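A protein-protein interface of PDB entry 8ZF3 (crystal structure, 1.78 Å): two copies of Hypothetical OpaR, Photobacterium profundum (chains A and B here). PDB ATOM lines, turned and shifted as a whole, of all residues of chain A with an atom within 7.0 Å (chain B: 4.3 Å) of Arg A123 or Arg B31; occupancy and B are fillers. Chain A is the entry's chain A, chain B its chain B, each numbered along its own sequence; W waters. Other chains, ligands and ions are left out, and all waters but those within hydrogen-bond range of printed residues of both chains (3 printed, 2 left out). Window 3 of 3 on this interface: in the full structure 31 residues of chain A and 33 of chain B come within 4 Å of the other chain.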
ATOM      1  N   THR A 120     -15.805  11.485   7.534  1.00  0.00           N
ATOM      2  CA  THR A 120     -15.568  12.812   8.093  1.00  0.00           C
ATOM      3  C   THR A 120     -14.388  12.842   9.056  1.00  0.00           C
ATOM      4  O   THR A 120     -14.166  13.863   9.710  1.00  0.00           O
ATOM      5  CB  THR A 120     -16.835  13.327   8.791  1.00  0.00           C
ATOM      6  OG1 THR A 120     -17.259  12.370   9.771  1.00  0.00           O
ATOM      7  CG2 THR A 120     -17.962  13.474   7.777  1.00  0.00           C
ATOM      8  N   SER A 121     -13.617  11.756   9.144  1.00  0.00           N
ATOM      9  CA  SER A 121     -12.447  11.690  10.019  1.00  0.00           C
ATOM     10  C   SER A 121     -11.207  12.277   9.343  1.00  0.00           C
ATOM     11  O   SER A 121     -10.157  11.625   9.295  1.00  0.00           O
ATOM     12  CB  SER A 121     -12.183  10.235  10.418  1.00  0.00           C
ATOM     13  OG  SER A 121     -13.204   9.778  11.295  1.00  0.00           O
ATOM     14  N   VAL A 122     -11.296  13.512   8.838  1.00  0.00           N
ATOM     15  CA  VAL A 122     -10.335  13.964   7.829  1.00  0.00           C
ATOM     16  C   VAL A 122      -8.940  14.230   8.374  1.00  0.00           C
ATOM     17  O   VAL A 122      -7.996  14.356   7.586  1.00  0.00           O
ATOM     18  CB  VAL A 122     -10.842  15.230   7.117  1.00  0.00           C
ATOM     19  CG1 VAL A 122     -12.162  14.944   6.427  1.00  0.00           C
ATOM     20  CG2 VAL A 122     -10.971  16.360   8.101  1.00  0.00           C
ATOM     21  N   ARG A 123      -8.779  14.343   9.685  1.00  0.00           N
ATOM     22  CA  ARG A 123      -7.478  14.602  10.290  1.00  0.00           C
ATOM     23  C   ARG A 123      -6.857  13.362  10.906  1.00  0.00           C
ATOM     24  O   ARG A 123      -5.731  13.431  11.416  1.00  0.00           O
ATOM     25  CB  ARG A 123      -7.598  15.680  11.358  1.00  0.00           C
ATOM     26  CG  ARG A 123      -7.908  17.036  10.821  1.00  0.00           C
ATOM     27  CD  ARG A 123      -7.664  18.044  11.909  1.00  0.00           C
ATOM     28  NE  ARG A 123      -8.244  19.328  11.557  1.00  0.00           N
ATOM     29  CZ  ARG A 123      -8.200  20.400  12.329  1.00  0.00           C
ATOM     30  NH1 ARG A 123      -7.662  20.355  13.537  1.00  0.00           N
ATOM     31  NH2 ARG A 123      -8.717  21.543  11.883  1.00  0.00           N
ATOM     32  N   ASP A 124      -7.576  12.247  10.890  1.00  0.00           N
ATOM     33  CA  ASP A 124      -7.066  11.001  11.419  1.00  0.00           C
ATOM     34  C   ASP A 124      -6.207  10.289  10.370  1.00  0.00           C
ATOM     35  O   ASP A 124      -6.365  10.471   9.158  1.00  0.00           O
ATOM     36  CB  ASP A 124      -8.224  10.106  11.842  1.00  0.00           C
ATOM     37  CG  ASP A 124      -7.769   8.941  12.682  1.00  0.00           C
ATOM     38  OD1 ASP A 124      -7.118   8.016  12.141  1.00  0.00           O
ATOM     39  OD2 ASP A 124      -8.090   8.936  13.885  1.00  0.00           O
ATOM     40  N   ASP A 125      -5.304   9.440  10.859  1.00  0.00           N
ATOM     41  CA  ASP A 125      -4.422   8.663   9.999  1.00  0.00           C
ATOM     42  C   ASP A 125      -5.161   7.593   9.205  1.00  0.00           C
ATOM     43  O   ASP A 125      -4.575   7.026   8.276  1.00  0.00           O
ATOM     44  CB  ASP A 125      -3.336   7.991  10.840  1.00  0.00           C
ATOM     45  CG  ASP A 125      -2.296   8.968  11.365  1.00  0.00           C
ATOM     46  OD1 ASP A 125      -2.247  10.138  10.917  1.00  0.00           O
ATOM     47  OD2 ASP A 125      -1.523   8.554  12.245  1.00  0.00           O
ATOM     48  N   ILE A 126      -6.414   7.288   9.555  1.00  0.00           N
ATOM     49  CA  ILE A 126      -7.201   6.314   8.795  1.00  0.00           C
ATOM     50  C   ILE A 126      -7.827   6.936   7.564  1.00  0.00           C
ATOM     51  O   ILE A 126      -8.455   6.212   6.761  1.00  0.00           O
ATOM     52  CB  ILE A 126      -8.323   5.672   9.637  1.00  0.00           C
ATOM     53  CG1 ILE A 126      -9.317   6.736  10.135  1.00  0.00           C
ATOM     54  CG2 ILE A 126      -7.759   4.830  10.789  1.00  0.00           C
ATOM     55  CD1 ILE A 126     -10.586   6.181  10.773  1.00  0.00           C
ATOM     56  N   TRP A 127      -7.620   8.263   7.347  1.00  0.00           N
ATOM     57  CA  TRP A 127      -8.391   8.923   6.265  1.00  0.00           C
ATOM     58  C   TRP A 127      -7.801   8.713   4.860  1.00  0.00           C
ATOM     59  O   TRP A 127      -8.644   8.412   3.995  1.00  0.00           O
ATOM     60  CB  TRP A 127      -8.619  10.424   6.602  1.00  0.00           C
ATOM     61  CG  TRP A 127      -9.797  11.059   5.833  1.00  0.00           C
ATOM     62  CD1 TRP A 127     -11.120  10.736   5.919  1.00  0.00           C
ATOM     63  CD2 TRP A 127      -9.693  11.970   4.728  1.00  0.00           C
ATOM     64  NE1 TRP A 127     -11.875  11.509   5.046  1.00  0.00           N
ATOM     65  CE2 TRP A 127     -11.007  12.256   4.291  1.00  0.00           C
ATOM     66  CE3 TRP A 127      -8.618  12.618   4.106  1.00  0.00           C
ATOM     67  CZ2 TRP A 127     -11.269  13.155   3.260  1.00  0.00           C
ATOM     68  CZ3 TRP A 127      -8.885  13.496   3.080  1.00  0.00           C
ATOM     69  CH2 TRP A 127     -10.195  13.753   2.664  1.00  0.00           C
ATOM     70  N   ASP B  27     -10.241  23.721  19.276  1.00  0.00           N
ATOM     71  CA  ASP B  27      -8.963  23.241  18.753  1.00  0.00           C
ATOM     72  C   ASP B  27      -8.731  21.779  19.130  1.00  0.00           C
ATOM     73  O   ASP B  27      -8.381  20.948  18.281  1.00  0.00           O
ATOM     74  CB  ASP B  27      -7.837  24.137  19.293  1.00  0.00           C
ATOM     75  CG  ASP B  27      -6.457  23.804  18.728  1.00  0.00           C
ATOM     76  OD1 ASP B  27      -6.010  22.635  18.781  1.00  0.00           O
ATOM     77  OD2 ASP B  27      -5.755  24.754  18.331  1.00  0.00           O
ATOM     78  N   VAL B  28      -8.941  21.446  20.405  1.00  0.00           N
ATOM     79  CA  VAL B  28      -8.717  20.081  20.879  1.00  0.00           C
ATOM     80  C   VAL B  28      -9.721  19.118  20.247  1.00  0.00           C
ATOM     81  O   VAL B  28      -9.363  18.007  19.833  1.00  0.00           O
ATOM     82  CB  VAL B  28      -8.790  20.050  22.420  1.00  0.00           C
ATOM     83  CG1 VAL B  28      -8.761  18.609  22.936  1.00  0.00           C
ATOM     84  CG2 VAL B  28      -7.643  20.878  23.041  1.00  0.00           C
ATOM     85  N   PHE B  29     -10.992  19.520  20.166  1.00  0.00           N
ATOM     86  CA  PHE B  29     -12.002  18.627  19.590  1.00  0.00           C
ATOM     87  C   PHE B  29     -11.756  18.391  18.116  1.00  0.00           C
ATOM     88  O   PHE B  29     -12.011  17.293  17.613  1.00  0.00           O
ATOM     89  CB  PHE B  29     -13.404  19.188  19.771  1.00  0.00           C
ATOM     90  CG  PHE B  29     -13.908  19.088  21.161  1.00  0.00           C
ATOM     91  CD1 PHE B  29     -13.114  18.546  22.157  1.00  0.00           C
ATOM     92  CD2 PHE B  29     -15.146  19.609  21.497  1.00  0.00           C
ATOM     93  CE1 PHE B  29     -13.563  18.463  23.466  1.00  0.00           C
ATOM     94  CE2 PHE B  29     -15.599  19.545  22.813  1.00  0.00           C
ATOM     95  CZ  PHE B  29     -14.801  18.978  23.793  1.00  0.00           C
ATOM     96  N   ALA B  30     -11.301  19.420  17.398  1.00  0.00           N
ATOM     97  CA  ALA B  30     -11.008  19.206  15.983  1.00  0.00           C
ATOM     98  C   ALA B  30      -9.851  18.232  15.802  1.00  0.00           C
ATOM     99  O   ALA B  30      -9.847  17.447  14.847  1.00  0.00           O
ATOM    100  CB  ALA B  30     -10.699  20.531  15.282  1.00  0.00           C
ATOM    101  N   ARG B  31      -8.870  18.256  16.707  1.00  0.00           N
ATOM    102  CA  ARG B  31      -7.722  17.372  16.568  1.00  0.00           C
ATOM    103  C   ARG B  31      -8.044  15.954  17.020  1.00  0.00           C
ATOM    104  O   ARG B  31      -7.657  14.989  16.352  1.00  0.00           O
ATOM    105  CB  ARG B  31      -6.520  17.920  17.354  1.00  0.00           C
ATOM    106  CG  ARG B  31      -5.806  19.099  16.691  1.00  0.00           C
ATOM    107  CD  ARG B  31      -4.813  19.743  17.656  1.00  0.00           C
ATOM    108  NE  ARG B  31      -4.633  18.915  18.842  1.00  0.00           N
ATOM    109  CZ  ARG B  31      -4.729  19.354  20.088  1.00  0.00           C
ATOM    110  NH1 ARG B  31      -5.037  20.615  20.355  1.00  0.00           N
ATOM    111  NH2 ARG B  31      -4.515  18.505  21.092  1.00  0.00           N
ATOM    112  N   ARG B  32      -8.759  15.803  18.134  1.00  0.00           N
ATOM    113  CA  ARG B  32      -8.915  14.501  18.766  1.00  0.00           C
ATOM    114  C   ARG B  32     -10.337  13.947  18.708  1.00  0.00           C
ATOM    115  O   ARG B  32     -10.538  12.780  19.055  1.00  0.00           O
ATOM    116  CB  ARG B  32      -8.471  14.571  20.235  1.00  0.00           C
ATOM    117  CG  ARG B  32      -6.972  14.785  20.419  1.00  0.00           C
ATOM    118  CD  ARG B  32      -6.579  14.907  21.887  1.00  0.00           C
ATOM    119  NE  ARG B  32      -7.004  13.744  22.665  1.00  0.00           N
ATOM    120  CZ  ARG B  32      -7.520  13.794  23.889  1.00  0.00           C
ATOM    121  NH1 ARG B  32      -7.741  14.946  24.501  1.00  0.00           N
ATOM    122  NH2 ARG B  32      -7.838  12.657  24.509  1.00  0.00           N
ATOM    123  N   GLY B  33     -11.320  14.738  18.313  1.00  0.00           N
ATOM    124  CA  GLY B  33     -12.686  14.238  18.289  1.00  0.00           C
ATOM    125  C   GLY B  33     -13.516  14.877  19.384  1.00  0.00           C
ATOM    126  O   GLY B  33     -13.042  15.109  20.504  1.00  0.00           O
ATOM    127  N   MET B  45      -3.333  24.217  27.330  1.00  0.00           N
ATOM    128  CA  MET B  45      -3.305  25.257  26.300  1.00  0.00           C
ATOM    129  C   MET B  45      -3.508  26.634  26.918  1.00  0.00           C
ATOM    130  O   MET B  45      -2.883  27.616  26.506  1.00  0.00           O
ATOM    131  CB  MET B  45      -4.406  25.020  25.258  1.00  0.00           C
ATOM    132  CG  MET B  45      -4.205  23.863  24.313  1.00  0.00           C
ATOM    133  SD  MET B  45      -5.225  23.963  22.810  1.00  0.00           S
ATOM    134  CE  MET B  45      -4.551  25.393  21.948  1.00  0.00           C
ATOM    135  N   GLN B 108      -8.073  25.294   7.274  1.00  0.00           N
ATOM    136  CA  GLN B 108      -8.245  24.279   8.324  1.00  0.00           C
ATOM    137  C   GLN B 108      -8.968  24.859   9.539  1.00  0.00           C
ATOM    138  O   GLN B 108      -8.518  24.754  10.691  1.00  0.00           O
ATOM    139  CB  GLN B 108      -6.893  23.649   8.704  1.00  0.00           C
ATOM    140  CG  GLN B 108      -6.322  22.707   7.618  1.00  0.00           C
ATOM    141  CD  GLN B 108      -7.123  21.404   7.466  1.00  0.00           C
ATOM    142  OE1 GLN B 108      -7.023  20.501   8.308  1.00  0.00           O
ATOM    143  NE2 GLN B 108      -7.935  21.310   6.410  1.00  0.00           N
ATOM    144  N   ASP B 110     -11.303  25.036  12.505  1.00  0.00           N
ATOM    145  CA  ASP B 110     -11.687  23.963  13.424  1.00  0.00           C
ATOM    146  C   ASP B 110     -13.193  23.758  13.448  1.00  0.00           C
ATOM    147  O   ASP B 110     -13.672  22.617  13.508  1.00  0.00           O
ATOM    148  CB  ASP B 110     -11.211  24.279  14.840  1.00  0.00           C
ATOM    149  CG  ASP B 110      -9.701  24.169  15.002  1.00  0.00           C
ATOM    150  OD1 ASP B 110      -9.056  23.395  14.263  1.00  0.00           O
ATOM    151  OD2 ASP B 110      -9.176  24.825  15.917  1.00  0.00           O
ATOM    152  N   LYS B 113     -14.578  21.381  10.663  1.00  0.00           N
ATOM    153  CA  LYS B 113     -14.249  19.975  10.889  1.00  0.00           C
ATOM    154  C   LYS B 113     -15.161  19.370  11.951  1.00  0.00           C
ATOM    155  O   LYS B 113     -15.698  18.269  11.771  1.00  0.00           O
ATOM    156  CB  LYS B 113     -12.784  19.837  11.308  1.00  0.00           C
ATOM    157  CG  LYS B 113     -12.280  18.378  11.332  1.00  0.00           C
ATOM    158  CD  LYS B 113     -12.205  17.797  12.751  1.00  0.00           C
ATOM    159  CE  LYS B 113     -11.808  16.333  12.723  1.00  0.00           C
ATOM    160  NZ  LYS B 113     -12.402  15.687  11.514  1.00  0.00           N
HETATM  161  O   HOH W   1     -14.775  16.494   9.707  1.00  0.00           O
HETATM  162  O   HOH W   2      -6.481  23.950  12.520  1.00  0.00           O
HETATM  163  O   HOH W   3      -7.112  21.858  15.844  1.00  0.00           O
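The backbone carbonyl oxygen of Thr A120 sits at hydrogen-bond distance from the side-chain amino group of Lys B113 (3.1 Å).
O of Gln B108 sits at hydrogen-bond distance from NH2 of Arg A123 (3.4 Å).
The guanidinium group of Arg A123 lies within salt-bridge range of the side-chain carboxylate of Asp B110 (3.0 Å).
NH1 of Arg B31 is in salt-bridge range of OD1 of Asp B27 (2.7 Å).
N of Val A122 touches NZ of Lys B113, 3.6 Å away.
NH1 of Arg A123 touches CB of Ala B30, 3.5 Å away.
Arg A123 touches Arg B31.
Printed residues of chain B within 4 Å of Val A122: Lys B113 (3.6 Å).
Arg A123 touches four residues of chain B.
Phe B29 touches none of the printed residues of chain A.
Of the printed residues of chain A, Ala B30 touches Arg A123.
Arg B31 touches just one residue of chain A: Arg A123 (3.9 Å).
Printed residues of chain A within 4 Å of Gln B108: Arg A123 (3.4 Å).
Of the printed residues of chain A, Asp B110 touches Arg A123 (3.0 Å).
Printed residues of chain A within 4 Å of Lys B113: Thr A120 and Val A122.
The nearest residue of chain B that does not touch Arg A123 is Lys B113 (4.2 Å).
The nearest printed residue of chain A that does not touch Ala B30 is Asp A124 (6.9 Å).
Along chain B the printed residues that touch a printed residue of chain A span positions 30 to 113.
Hydrophobic or aromatic side chains of chain A that line the printed part of chain B: Val A122.
No position is printed for both chains.
Of the 6 pairs that touch across the chains among the printed residues, none has its exchanged pair printed and touching as well.
Water W1 lies within hydrogen-bond range of the backbone carbonyl oxygen of Thr A120 (2.7 Å) and the backbone carbonyl oxygen of Lys B113 (2.9 Å).
Water W3 lies within hydrogen-bond range of the guanidinium group of Arg A123, the backbone carbonyl oxygen of Asp B27 and the side-chain carboxylate of Asp B110.
Water W2 lies within hydrogen-bond range of the backbone carbonyl oxygen of Gln B108 (2.9 Å), the side-chain carboxylate of Asp B110 (3.2 Å) and the guanidinium group of Arg A123 (3.3 Å).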
